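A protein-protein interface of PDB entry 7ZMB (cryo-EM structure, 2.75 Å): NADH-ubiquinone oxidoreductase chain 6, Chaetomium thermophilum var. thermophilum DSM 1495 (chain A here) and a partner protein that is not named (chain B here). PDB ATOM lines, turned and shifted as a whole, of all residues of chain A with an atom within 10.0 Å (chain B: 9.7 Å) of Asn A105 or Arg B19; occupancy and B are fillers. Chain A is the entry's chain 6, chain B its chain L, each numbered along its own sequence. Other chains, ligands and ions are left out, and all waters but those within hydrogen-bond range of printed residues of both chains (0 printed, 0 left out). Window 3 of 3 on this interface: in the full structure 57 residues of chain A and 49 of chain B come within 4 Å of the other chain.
Of the printed residues of chain B, Val A37 touches Leu B24.
Of the printed residues of chain B, Ile A38 touches Gly B14 and Lys B20.
No residue of chain B comes within 4 Å of Thr A103.
No residue of chain B comes within 4 Å of Ser A104.
Of chain B, only Arg B19 (3.9 Å) comes within 4 Å of Asn A105.
Of chain B, only Leu B17 comes within 4 Å of Ser A106.
Of the printed residues of chain B, Leu A109 touches Leu B17.
No residue of chain A comes within 4 Å of Asn B18.
Arg B19 touches just these residues of chain A: Gln A100 and Asn A105.
Ser B28 touches none of the printed residues of chain A.
Ile B84 touches none of the printed residues of chain A.
The nearest residue of chain A that does not touch Arg B19 is Ser A106 (4.1 Å).
The nearest printed residue of chain A that does not touch Gly B14 is Val A37 (7.3 Å).
Of the 21 printed residues of chain A, 9 touch a printed residue of chain B.
Among the printed residues, 12 pairs touch across the chains.
Among the printed residues, no Asp or Glu carboxylate lies within 4 Å of a Lys or Arg side-chain nitrogen of the other chain.
O of Ser A106 is in hydrogen-bond range of OG1 of Thr A110 (2.5 Å).
The side-chain amide oxygen (OD1) of Asn B18 is in hydrogen-bond range of the backbone NH (N) of Lys B20, 2.8 Å away.
The backbone carbonyl oxygen (O) of Gly B14 sits at hydrogen-bond distance from the side-chain hydroxyl (OG) of Ser B28.
N of Ile B86 is in hydrogen-bond range of O of Lys B20, at 3.5 Å.
The backbone carbonyl oxygen (O) of Leu B24 is in hydrogen-bond range of the side-chain hydroxyl (OG) of Ser B28 (3.0 Å).
The backbone NH (N) of Leu B24 sits at hydrogen-bond distance from the side-chain amide oxygen (OD1) of Asn B21, at 2.9 Å.
Among the printed residues, merely in contact across the chains: Ser A106 with Leu B17 (3.3 Å), Ile A38 with Lys B20 (3.4 Å), Val A37 with Leu B24 (3.4 Å), Gln A100 with Arg B19 (3.5 Å), Thr A110 with Leu B13 (3.6 Å), Lys A41 with Lys B20 (3.6 Å), Ile A38 with Gly B14 (3.7 Å), Asn A105 with Arg B19 (3.9 Å), Gln A100 with Ile B86 (3.9 Å) and Leu A109 with Leu B17 (3.96 Å).
The backbone carbonyl oxygen (O) of Lys B20 lies within hydrogen-bond range of the side-chain amide nitrogen (NE2) of Gln A100, 2.4 Å away.
NZ of Lys B20 sits at hydrogen-bond distance from O of Ser A40 (3.1 Å).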
ATOM      1  N   VAL A  37     -32.843  -6.109 -27.663  1.00  0.00           N
ATOM      2  CA  VAL A  37     -32.046  -5.892 -26.459  1.00  0.00           C
ATOM      3  C   VAL A  37     -31.460  -7.200 -25.940  1.00  0.00           C
ATOM      4  O   VAL A  37     -30.393  -7.208 -25.318  1.00  0.00           O
ATOM      5  CB  VAL A  37     -32.894  -5.178 -25.387  1.00  0.00           C
ATOM      6  CG1 VAL A  37     -32.139  -5.051 -24.083  1.00  0.00           C
ATOM      7  CG2 VAL A  37     -33.292  -3.794 -25.871  1.00  0.00           C
ATOM      8  N   ILE A  38     -32.123  -8.325 -26.194  1.00  0.00           N
ATOM      9  CA  ILE A  38     -31.692  -9.595 -25.631  1.00  0.00           C
ATOM     10  C   ILE A  38     -31.149 -10.564 -26.671  1.00  0.00           C
ATOM     11  O   ILE A  38     -30.338 -11.431 -26.312  1.00  0.00           O
ATOM     12  CB  ILE A  38     -32.822 -10.256 -24.816  1.00  0.00           C
ATOM     13  CG1 ILE A  38     -34.090 -10.379 -25.652  1.00  0.00           C
ATOM     14  CG2 ILE A  38     -33.109  -9.446 -23.561  1.00  0.00           C
ATOM     15  CD1 ILE A  38     -35.266 -10.891 -24.891  1.00  0.00           C
ATOM     16  N   ILE A  39     -31.539 -10.443 -27.943  1.00  0.00           N
ATOM     17  CA  ILE A  39     -31.024 -11.356 -28.959  1.00  0.00           C
ATOM     18  C   ILE A  39     -29.713 -10.889 -29.572  1.00  0.00           C
ATOM     19  O   ILE A  39     -29.023 -11.694 -30.214  1.00  0.00           O
ATOM     20  CB  ILE A  39     -32.043 -11.593 -30.094  1.00  0.00           C
ATOM     21  CG1 ILE A  39     -32.200 -10.339 -30.956  1.00  0.00           C
ATOM     22  CG2 ILE A  39     -33.374 -12.052 -29.533  1.00  0.00           C
ATOM     23  CD1 ILE A  39     -33.085 -10.540 -32.149  1.00  0.00           C
ATOM     24  N   SER A  40     -29.333  -9.630 -29.386  1.00  0.00           N
ATOM     25  CA  SER A  40     -28.152  -9.085 -30.040  1.00  0.00           C
ATOM     26  C   SER A  40     -26.877  -9.647 -29.430  1.00  0.00           C
ATOM     27  O   SER A  40     -26.782  -9.834 -28.219  1.00  0.00           O
ATOM     28  CB  SER A  40     -28.143  -7.562 -29.942  1.00  0.00           C
ATOM     29  OG  SER A  40     -29.003  -6.988 -30.907  1.00  0.00           O
ATOM     30  N   LYS A  41     -25.885  -9.899 -30.279  1.00  0.00           N
ATOM     31  CA  LYS A  41     -24.644 -10.499 -29.809  1.00  0.00           C
ATOM     32  C   LYS A  41     -23.700  -9.468 -29.209  1.00  0.00           C
ATOM     33  O   LYS A  41     -22.835  -9.825 -28.405  1.00  0.00           O
ATOM     34  CB  LYS A  41     -23.969 -11.249 -30.960  1.00  0.00           C
ATOM     35  CG  LYS A  41     -24.741 -12.494 -31.373  1.00  0.00           C
ATOM     36  CD  LYS A  41     -24.167 -13.175 -32.611  1.00  0.00           C
ATOM     37  CE  LYS A  41     -22.837 -13.849 -32.337  1.00  0.00           C
ATOM     38  NZ  LYS A  41     -22.359 -14.602 -33.530  1.00  0.00           N
ATOM     39  N   THR A  96     -15.135 -10.938 -26.915  1.00  0.00           N
ATOM     40  CA  THR A  96     -15.441 -12.314 -26.530  1.00  0.00           C
ATOM     41  C   THR A  96     -16.942 -12.513 -26.353  1.00  0.00           C
ATOM     42  O   THR A  96     -17.449 -13.625 -26.521  1.00  0.00           O
ATOM     43  CB  THR A  96     -14.697 -12.708 -25.248  1.00  0.00           C
ATOM     44  OG1 THR A  96     -15.104 -11.874 -24.164  1.00  0.00           O
ATOM     45  CG2 THR A  96     -13.211 -12.561 -25.422  1.00  0.00           C
ATOM     46  N   SER A  97     -17.670 -11.448 -26.023  1.00  0.00           N
ATOM     47  CA  SER A  97     -19.117 -11.565 -25.887  1.00  0.00           C
ATOM     48  C   SER A  97     -19.809 -11.607 -27.248  1.00  0.00           C
ATOM     49  O   SER A  97     -20.831 -12.279 -27.408  1.00  0.00           O
ATOM     50  CB  SER A  97     -19.659 -10.424 -25.027  1.00  0.00           C
ATOM     51  OG  SER A  97     -19.879  -9.264 -25.790  1.00  0.00           O
ATOM     52  N   GLU A  98     -19.274 -10.902 -28.244  1.00  0.00           N
ATOM     53  CA  GLU A  98     -19.824 -11.043 -29.591  1.00  0.00           C
ATOM     54  C   GLU A  98     -19.583 -12.428 -30.167  1.00  0.00           C
ATOM     55  O   GLU A  98     -20.152 -12.756 -31.211  1.00  0.00           O
ATOM     56  CB  GLU A  98     -19.233 -10.004 -30.540  1.00  0.00           C
ATOM     57  CG  GLU A  98     -19.713  -8.607 -30.305  1.00  0.00           C
ATOM     58  CD  GLU A  98     -18.998  -7.604 -31.183  1.00  0.00           C
ATOM     59  OE1 GLU A  98     -17.758  -7.701 -31.310  1.00  0.00           O
ATOM     60  OE2 GLU A  98     -19.677  -6.726 -31.757  1.00  0.00           O
ATOM     61  N   LEU A  99     -18.732 -13.220 -29.527  1.00  0.00           N
ATOM     62  CA  LEU A  99     -18.523 -14.619 -29.851  1.00  0.00           C
ATOM     63  C   LEU A  99     -19.298 -15.538 -28.921  1.00  0.00           C
ATOM     64  O   LEU A  99     -19.206 -16.761 -29.044  1.00  0.00           O
ATOM     65  CB  LEU A  99     -17.029 -14.930 -29.786  1.00  0.00           C
ATOM     66  CG  LEU A  99     -16.268 -14.041 -30.759  1.00  0.00           C
ATOM     67  CD1 LEU A  99     -14.807 -13.894 -30.395  1.00  0.00           C
ATOM     68  CD2 LEU A  99     -16.424 -14.689 -32.091  1.00  0.00           C
ATOM     69  N   GLN A 100     -20.061 -14.965 -27.993  1.00  0.00           N
ATOM     70  CA  GLN A 100     -20.798 -15.713 -26.981  1.00  0.00           C
ATOM     71  C   GLN A 100     -22.124 -16.217 -27.560  1.00  0.00           C
ATOM     72  O   GLN A 100     -23.215 -15.896 -27.090  1.00  0.00           O
ATOM     73  CB  GLN A 100     -21.012 -14.818 -25.767  1.00  0.00           C
ATOM     74  CG  GLN A 100     -21.173 -15.500 -24.427  1.00  0.00           C
ATOM     75  CD  GLN A 100     -21.519 -14.500 -23.341  1.00  0.00           C
ATOM     76  OE1 GLN A 100     -21.724 -13.322 -23.623  1.00  0.00           O
ATOM     77  NE2 GLN A 100     -21.578 -14.959 -22.102  1.00  0.00           N
ATOM     78  N   SER A 101     -22.004 -17.022 -28.614  1.00  0.00           N
ATOM     79  CA  SER A 101     -23.174 -17.463 -29.360  1.00  0.00           C
ATOM     80  C   SER A 101     -24.048 -18.377 -28.513  1.00  0.00           C
ATOM     81  O   SER A 101     -23.554 -19.162 -27.699  1.00  0.00           O
ATOM     82  CB  SER A 101     -22.745 -18.181 -30.642  1.00  0.00           C
ATOM     83  OG  SER A 101     -21.989 -19.343 -30.350  1.00  0.00           O
ATOM     84  N   ASN A 102     -25.359 -18.271 -28.713  1.00  0.00           N
ATOM     85  CA  ASN A 102     -26.333 -19.054 -27.972  1.00  0.00           C
ATOM     86  C   ASN A 102     -27.175 -19.867 -28.944  1.00  0.00           C
ATOM     87  O   ASN A 102     -27.373 -19.477 -30.097  1.00  0.00           O
ATOM     88  CB  ASN A 102     -27.241 -18.162 -27.115  1.00  0.00           C
ATOM     89  N   THR A 103     -27.668 -21.005 -28.465  1.00  0.00           N
ATOM     90  CA  THR A 103     -28.449 -21.922 -29.280  1.00  0.00           C
ATOM     91  C   THR A 103     -29.931 -21.707 -29.016  1.00  0.00           C
ATOM     92  O   THR A 103     -30.326 -20.983 -28.099  1.00  0.00           O
ATOM     93  CB  THR A 103     -28.085 -23.385 -29.004  1.00  0.00           C
ATOM     94  N   SER A 104     -30.786 -22.265 -29.867  1.00  0.00           N
ATOM     95  CA  SER A 104     -32.230 -22.119 -29.544  1.00  0.00           C
ATOM     96  C   SER A 104     -32.777 -23.420 -28.956  1.00  0.00           C
ATOM     97  O   SER A 104     -33.778 -23.938 -29.489  1.00  0.00           O
ATOM     98  CB  SER A 104     -33.028 -21.690 -30.736  1.00  0.00           C
ATOM     99  N   ASN A 105     -32.156 -23.918 -27.879  1.00  0.00           N
ATOM    100  CA  ASN A 105     -32.719 -25.108 -27.183  1.00  0.00           C
ATOM    101  C   ASN A 105     -33.837 -24.571 -26.288  1.00  0.00           C
ATOM    102  O   ASN A 105     -34.650 -25.373 -25.809  1.00  0.00           O
ATOM    103  CB  ASN A 105     -31.638 -25.905 -26.445  1.00  0.00           C
ATOM    104  CG  ASN A 105     -30.957 -25.123 -25.343  1.00  0.00           C
ATOM    105  OD1 ASN A 105     -31.095 -23.905 -25.261  1.00  0.00           O
ATOM    106  ND2 ASN A 105     -30.215 -25.813 -24.491  1.00  0.00           N
ATOM    107  N   SER A 106     -33.898 -23.249 -26.137  1.00  0.00           N
ATOM    108  CA  SER A 106     -34.885 -22.634 -25.222  1.00  0.00           C
ATOM    109  C   SER A 106     -36.095 -22.101 -25.982  1.00  0.00           C
ATOM    110  O   SER A 106     -36.963 -21.542 -25.305  1.00  0.00           O
ATOM    111  CB  SER A 106     -34.236 -21.556 -24.412  1.00  0.00           C
ATOM    112  OG  SER A 106     -33.374 -20.756 -25.189  1.00  0.00           O
ATOM    113  N   ILE A 107     -36.173 -22.304 -27.299  1.00  0.00           N
ATOM    114  CA  ILE A 107     -37.370 -21.890 -28.023  1.00  0.00           C
ATOM    115  C   ILE A 107     -38.608 -22.634 -27.530  1.00  0.00           C
ATOM    116  O   ILE A 107     -39.641 -21.987 -27.308  1.00  0.00           O
ATOM    117  CB  ILE A 107     -37.193 -22.065 -29.539  1.00  0.00           C
ATOM    118  CG1 ILE A 107     -36.008 -21.236 -30.024  1.00  0.00           C
ATOM    119  CG2 ILE A 107     -38.462 -21.674 -30.283  1.00  0.00           C
ATOM    120  CD1 ILE A 107     -36.174 -19.756 -29.785  1.00  0.00           C
ATOM    121  N   PRO A 108     -38.592 -23.967 -27.365  1.00  0.00           N
ATOM    122  CA  PRO A 108     -39.827 -24.626 -26.905  1.00  0.00           C
ATOM    123  C   PRO A 108     -40.282 -24.162 -25.537  1.00  0.00           C
ATOM    124  O   PRO A 108     -41.487 -24.089 -25.280  1.00  0.00           O
ATOM    125  CB  PRO A 108     -39.471 -26.118 -26.915  1.00  0.00           C
ATOM    126  CG  PRO A 108     -38.170 -26.232 -27.591  1.00  0.00           C
ATOM    127  CD  PRO A 108     -37.489 -24.929 -27.527  1.00  0.00           C
ATOM    128  N   LEU A 109     -39.348 -23.845 -24.645  1.00  0.00           N
ATOM    129  CA  LEU A 109     -39.735 -23.265 -23.367  1.00  0.00           C
ATOM    130  C   LEU A 109     -40.340 -21.883 -23.568  1.00  0.00           C
ATOM    131  O   LEU A 109     -41.318 -21.526 -22.905  1.00  0.00           O
ATOM    132  CB  LEU A 109     -38.525 -23.222 -22.431  1.00  0.00           C
ATOM    133  CG  LEU A 109     -38.717 -22.815 -20.972  1.00  0.00           C
ATOM    134  CD1 LEU A 109     -37.633 -23.459 -20.166  1.00  0.00           C
ATOM    135  CD2 LEU A 109     -38.632 -21.320 -20.783  1.00  0.00           C
ATOM    136  N   THR A 110     -39.776 -21.101 -24.494  1.00  0.00           N
ATOM    137  CA  THR A 110     -40.289 -19.766 -24.789  1.00  0.00           C
ATOM    138  C   THR A 110     -41.759 -19.809 -25.187  1.00  0.00           C
ATOM    139  O   THR A 110     -42.578 -19.039 -24.673  1.00  0.00           O
ATOM    140  CB  THR A 110     -39.460 -19.131 -25.907  1.00  0.00           C
ATOM    141  OG1 THR A 110     -38.062 -19.266 -25.615  1.00  0.00           O
ATOM    142  CG2 THR A 110     -39.805 -17.673 -26.072  1.00  0.00           C
ATOM    143  N   ILE A 111     -42.111 -20.721 -26.092  1.00  0.00           N
ATOM    144  CA  ILE A 111     -43.477 -20.783 -26.600  1.00  0.00           C
ATOM    145  C   ILE A 111     -44.450 -21.119 -25.478  1.00  0.00           C
ATOM    146  O   ILE A 111     -45.458 -20.431 -25.284  1.00  0.00           O
ATOM    147  CB  ILE A 111     -43.573 -21.800 -27.751  1.00  0.00           C
ATOM    148  CG1 ILE A 111     -42.487 -21.527 -28.790  1.00  0.00           C
ATOM    149  CG2 ILE A 111     -44.952 -21.752 -28.389  1.00  0.00           C
ATOM    150  CD1 ILE A 111     -42.594 -20.166 -29.436  1.00  0.00           C
ATOM    151  N   LEU B  13     -38.163 -13.304 -19.920  1.00  0.00           N
ATOM    152  CA  LEU B  13     -37.315 -14.279 -20.591  1.00  0.00           C
ATOM    153  C   LEU B  13     -35.908 -13.751 -20.807  1.00  0.00           C
ATOM    154  O   LEU B  13     -34.945 -14.515 -20.719  1.00  0.00           O
ATOM    155  CB  LEU B  13     -37.934 -14.696 -21.920  1.00  0.00           C
ATOM    156  CG  LEU B  13     -39.421 -15.027 -21.886  1.00  0.00           C
ATOM    157  CD1 LEU B  13     -39.879 -15.512 -23.232  1.00  0.00           C
ATOM    158  CD2 LEU B  13     -39.679 -16.086 -20.856  1.00  0.00           C
ATOM    159  N   GLY B  14     -35.765 -12.453 -21.067  1.00  0.00           N
ATOM    160  CA  GLY B  14     -34.442 -11.875 -21.138  1.00  0.00           C
ATOM    161  C   GLY B  14     -33.699 -11.905 -19.824  1.00  0.00           C
ATOM    162  O   GLY B  14     -32.495 -11.634 -19.805  1.00  0.00           O
ATOM    163  N   PHE B  15     -34.397 -12.194 -18.728  1.00  0.00           N
ATOM    164  CA  PHE B  15     -33.805 -12.438 -17.423  1.00  0.00           C
ATOM    165  C   PHE B  15     -33.558 -13.922 -17.197  1.00  0.00           C
ATOM    166  O   PHE B  15     -32.493 -14.309 -16.715  1.00  0.00           O
ATOM    167  CB  PHE B  15     -34.722 -11.876 -16.331  1.00  0.00           C
ATOM    168  CG  PHE B  15     -34.191 -12.030 -14.943  1.00  0.00           C
ATOM    169  CD1 PHE B  15     -33.294 -11.105 -14.423  1.00  0.00           C
ATOM    170  CD2 PHE B  15     -34.586 -13.096 -14.151  1.00  0.00           C
ATOM    171  CE1 PHE B  15     -32.801 -11.237 -13.141  1.00  0.00           C
ATOM    172  CE2 PHE B  15     -34.093 -13.240 -12.871  1.00  0.00           C
ATOM    173  CZ  PHE B  15     -33.200 -12.305 -12.364  1.00  0.00           C
ATOM    174  N   VAL B  16     -34.514 -14.765 -17.567  1.00  0.00           N
ATOM    175  CA  VAL B  16     -34.406 -16.187 -17.275  1.00  0.00           C
ATOM    176  C   VAL B  16     -33.727 -16.968 -18.392  1.00  0.00           C
ATOM    177  O   VAL B  16     -33.034 -17.953 -18.119  1.00  0.00           O
ATOM    178  CB  VAL B  16     -35.792 -16.763 -16.963  1.00  0.00           C
ATOM    179  CG1 VAL B  16     -35.650 -18.118 -16.432  1.00  0.00           C
ATOM    180  CG2 VAL B  16     -36.474 -15.919 -15.917  1.00  0.00           C
ATOM    181  N   LEU B  17     -33.897 -16.556 -19.643  1.00  0.00           N
ATOM    182  CA  LEU B  17     -33.304 -17.270 -20.761  1.00  0.00           C
ATOM    183  C   LEU B  17     -31.992 -16.638 -21.183  1.00  0.00           C
ATOM    184  O   LEU B  17     -31.452 -16.991 -22.234  1.00  0.00           O
ATOM    185  CB  LEU B  17     -34.265 -17.315 -21.952  1.00  0.00           C
ATOM    186  CG  LEU B  17     -35.395 -18.344 -21.878  1.00  0.00           C
ATOM    187  CD1 LEU B  17     -34.858 -19.753 -21.769  1.00  0.00           C
ATOM    188  CD2 LEU B  17     -36.413 -18.040 -20.780  1.00  0.00           C
ATOM    189  N   ASN B  18     -31.458 -15.734 -20.364  1.00  0.00           N
ATOM    190  CA  ASN B  18     -30.249 -14.981 -20.796  1.00  0.00           C
ATOM    191  C   ASN B  18     -28.993 -15.784 -20.476  1.00  0.00           C
ATOM    192  O   ASN B  18     -28.887 -16.248 -19.343  1.00  0.00           O
ATOM    193  CB  ASN B  18     -30.175 -13.633 -20.063  1.00  0.00           C
ATOM    194  CG  ASN B  18     -28.864 -12.892 -20.227  1.00  0.00           C
ATOM    195  OD1 ASN B  18     -28.137 -13.105 -21.191  1.00  0.00           O
ATOM    196  ND2 ASN B  18     -28.560 -12.013 -19.292  1.00  0.00           N
ATOM    197  N   ARG B  19     -28.119 -15.977 -21.463  1.00  0.00           N
ATOM    198  CA  ARG B  19     -26.886 -16.790 -21.280  1.00  0.00           C
ATOM    199  C   ARG B  19     -25.677 -15.940 -21.709  1.00  0.00           C
ATOM    200  O   ARG B  19     -24.713 -16.514 -22.254  1.00  0.00           O
ATOM    201  CB  ARG B  19     -27.049 -18.170 -21.930  1.00  0.00           C
ATOM    202  CG  ARG B  19     -27.888 -19.161 -21.137  1.00  0.00           C
ATOM    203  CD  ARG B  19     -29.390 -19.088 -21.380  1.00  0.00           C
ATOM    204  NE  ARG B  19     -30.191 -19.999 -20.569  1.00  0.00           N
ATOM    205  CZ  ARG B  19     -30.753 -21.118 -21.015  1.00  0.00           C
ATOM    206  NH1 ARG B  19     -31.455 -21.883 -20.195  1.00  0.00           N
ATOM    207  NH2 ARG B  19     -30.616 -21.463 -22.284  1.00  0.00           N
ATOM    208  N   LYS B  20     -25.747 -14.619 -21.484  1.00  0.00           N
ATOM    209  CA  LYS B  20     -24.665 -13.715 -21.940  1.00  0.00           C
ATOM    210  C   LYS B  20     -23.902 -13.091 -20.770  1.00  0.00           C
ATOM    211  O   LYS B  20     -22.703 -13.353 -20.647  1.00  0.00           O
ATOM    212  CB  LYS B  20     -25.249 -12.597 -22.799  1.00  0.00           C
ATOM    213  CG  LYS B  20     -25.780 -13.019 -24.158  1.00  0.00           C
ATOM    214  CD  LYS B  20     -26.435 -11.879 -24.887  1.00  0.00           C
ATOM    215  CE  LYS B  20     -27.058 -12.296 -26.202  1.00  0.00           C
ATOM    216  NZ  LYS B  20     -26.021 -12.642 -27.204  1.00  0.00           N
ATOM    217  N   ASN B  21     -24.558 -12.306 -19.928  1.00  0.00           N
ATOM    218  CA  ASN B  21     -23.861 -11.560 -18.888  1.00  0.00           C
ATOM    219  C   ASN B  21     -24.879 -10.934 -17.945  1.00  0.00           C
ATOM    220  O   ASN B  21     -26.070 -10.847 -18.250  1.00  0.00           O
ATOM    221  CB  ASN B  21     -22.927 -10.490 -19.476  1.00  0.00           C
ATOM    222  CG  ASN B  21     -23.650  -9.478 -20.336  1.00  0.00           C
ATOM    223  OD1 ASN B  21     -24.658  -8.906 -19.940  1.00  0.00           O
ATOM    224  ND2 ASN B  21     -23.144  -9.271 -21.540  1.00  0.00           N
ATOM    225  N   ILE B  22     -24.383 -10.484 -16.791  1.00  0.00           N
ATOM    226  CA  ILE B  22     -25.257 -10.027 -15.720  1.00  0.00           C
ATOM    227  C   ILE B  22     -25.760  -8.601 -15.932  1.00  0.00           C
ATOM    228  O   ILE B  22     -26.786  -8.226 -15.352  1.00  0.00           O
ATOM    229  CB  ILE B  22     -24.530 -10.176 -14.372  1.00  0.00           C
ATOM    230  CG1 ILE B  22     -24.033 -11.610 -14.200  1.00  0.00           C
ATOM    231  CG2 ILE B  22     -25.422  -9.801 -13.197  1.00  0.00           C
ATOM    232  CD1 ILE B  22     -22.777 -11.729 -13.379  1.00  0.00           C
ATOM    233  N   ILE B  23     -25.085  -7.783 -16.741  1.00  0.00           N
ATOM    234  CA  ILE B  23     -25.672  -6.484 -17.057  1.00  0.00           C
ATOM    235  C   ILE B  23     -26.950  -6.674 -17.863  1.00  0.00           C
ATOM    236  O   ILE B  23     -27.914  -5.923 -17.694  1.00  0.00           O
ATOM    237  CB  ILE B  23     -24.658  -5.567 -17.773  1.00  0.00           C
ATOM    238  CG1 ILE B  23     -23.498  -5.246 -16.841  1.00  0.00           C
ATOM    239  CG2 ILE B  23     -25.310  -4.260 -18.190  1.00  0.00           C
ATOM    240  CD1 ILE B  23     -22.599  -4.130 -17.302  1.00  0.00           C
ATOM    241  N   LEU B  24     -26.991  -7.684 -18.732  1.00  0.00           N
ATOM    242  CA  LEU B  24     -28.230  -7.987 -19.441  1.00  0.00           C
ATOM    243  C   LEU B  24     -29.277  -8.593 -18.520  1.00  0.00           C
ATOM    244  O   LEU B  24     -30.476  -8.416 -18.754  1.00  0.00           O
ATOM    245  CB  LEU B  24     -27.966  -8.920 -20.614  1.00  0.00           C
ATOM    246  CG  LEU B  24     -29.001  -8.750 -21.721  1.00  0.00           C
ATOM    247  CD1 LEU B  24     -29.102  -7.288 -22.130  1.00  0.00           C
ATOM    248  CD2 LEU B  24     -28.678  -9.632 -22.914  1.00  0.00           C
ATOM    249  N   MET B  25     -28.849  -9.324 -17.492  1.00  0.00           N
ATOM    250  CA  MET B  25     -29.757  -9.704 -16.415  1.00  0.00           C
ATOM    251  C   MET B  25     -30.400  -8.469 -15.804  1.00  0.00           C
ATOM    252  O   MET B  25     -31.626  -8.363 -15.711  1.00  0.00           O
ATOM    253  CB  MET B  25     -28.979 -10.470 -15.346  1.00  0.00           C
ATOM    254  CG  MET B  25     -28.425 -11.805 -15.768  1.00  0.00           C
ATOM    255  SD  MET B  25     -29.671 -12.980 -16.247  1.00  0.00           S
ATOM    256  CE  MET B  25     -30.404 -13.283 -14.644  1.00  0.00           C
ATOM    257  N   SER B  28     -32.882  -6.614 -18.003  1.00  0.00           N
ATOM    258  CA  SER B  28     -34.199  -7.211 -18.196  1.00  0.00           C
ATOM    259  C   SER B  28     -35.138  -6.907 -17.040  1.00  0.00           C
ATOM    260  O   SER B  28     -36.355  -6.840 -17.239  1.00  0.00           O
ATOM    261  CB  SER B  28     -34.062  -8.711 -18.396  1.00  0.00           C
ATOM    262  OG  SER B  28     -33.346  -8.965 -19.581  1.00  0.00           O
ATOM    263  N   ILE B  84     -17.996 -10.981 -15.680  1.00  0.00           N
ATOM    264  CA  ILE B  84     -19.423 -10.940 -15.237  1.00  0.00           C
ATOM    265  C   ILE B  84     -20.200 -11.717 -16.286  1.00  0.00           C
ATOM    266  O   ILE B  84     -21.413 -11.518 -16.395  1.00  0.00           O
ATOM    267  CB  ILE B  84     -19.941  -9.511 -15.011  1.00  0.00           C
ATOM    268  CG1 ILE B  84     -19.962  -8.699 -16.309  1.00  0.00           C
ATOM    269  CG2 ILE B  84     -19.152  -8.813 -13.920  1.00  0.00           C
ATOM    270  CD1 ILE B  84     -20.831  -7.475 -16.244  1.00  0.00           C
ATOM    271  N   ALA B  85     -19.498 -12.549 -17.044  1.00  0.00           N
ATOM    272  CA  ALA B  85     -20.114 -13.413 -18.035  1.00  0.00           C
ATOM    273  C   ALA B  85     -20.693 -14.621 -17.321  1.00  0.00           C
ATOM    274  O   ALA B  85     -20.051 -15.191 -16.431  1.00  0.00           O
ATOM    275  CB  ALA B  85     -19.099 -13.847 -19.089  1.00  0.00           C
ATOM    276  N   ILE B  86     -21.912 -14.995 -17.690  1.00  0.00           N
ATOM    277  CA  ILE B  86     -22.543 -16.151 -17.081  1.00  0.00           C
ATOM    278  C   ILE B  86     -22.242 -17.384 -17.921  1.00  0.00           C
ATOM    279  O   ILE B  86     -22.407 -17.384 -19.151  1.00  0.00           O
ATOM    280  CB  ILE B  86     -24.048 -15.890 -16.915  1.00  0.00           C
ATOM    281  CG1 ILE B  86     -24.716 -15.663 -18.262  1.00  0.00           C
ATOM    282  CG2 ILE B  86     -24.286 -14.668 -16.039  1.00  0.00           C
ATOM    283  CD1 ILE B  86     -26.185 -15.604 -18.137  1.00  0.00           C
ATOM    284  N   GLU B  87     -21.765 -18.439 -17.268  1.00  0.00           N
ATOM    285  CA  GLU B  87     -21.122 -19.548 -17.957  1.00  0.00           C
ATOM    286  C   GLU B  87     -22.046 -20.754 -18.022  1.00  0.00           C
ATOM    287  O   GLU B  87     -22.566 -21.203 -16.994  1.00  0.00           O
ATOM    288  CB  GLU B  87     -19.810 -19.930 -17.265  1.00  0.00           C
ATOM    289  CG  GLU B  87     -18.742 -18.852 -17.334  1.00  0.00           C
ATOM    290  CD  GLU B  87     -17.381 -19.349 -16.888  1.00  0.00           C
ATOM    291  OE1 GLU B  87     -17.175 -20.580 -16.858  1.00  0.00           O
ATOM    292  OE2 GLU B  87     -16.516 -18.508 -16.565  1.00  0.00           O
ATOM    293  N   TYR B  88     -22.237 -21.278 -19.230  1.00  0.00           N
ATOM    294  CA  TYR B  88     -22.943 -22.530 -19.456  1.00  0.00           C
ATOM    295  C   TYR B  88     -21.976 -23.524 -20.081  1.00  0.00           C
ATOM    296  O   TYR B  88     -21.281 -23.191 -21.046  1.00  0.00           O
ATOM    297  CB  TYR B  88     -24.160 -22.329 -20.361  1.00  0.00           C
ATOM    298  N   LYS B  89     -21.931 -24.732 -19.524  1.00  0.00           N
ATOM    299  CA  LYS B  89     -21.024 -25.782 -19.988  1.00  0.00           C
ATOM    300  C   LYS B  89     -19.568 -25.327 -19.947  1.00  0.00           C
ATOM    301  O   LYS B  89     -18.682 -26.001 -20.472  1.00  0.00           O
ATOM    302  CB  LYS B  89     -21.392 -26.230 -21.404  1.00  0.00           C
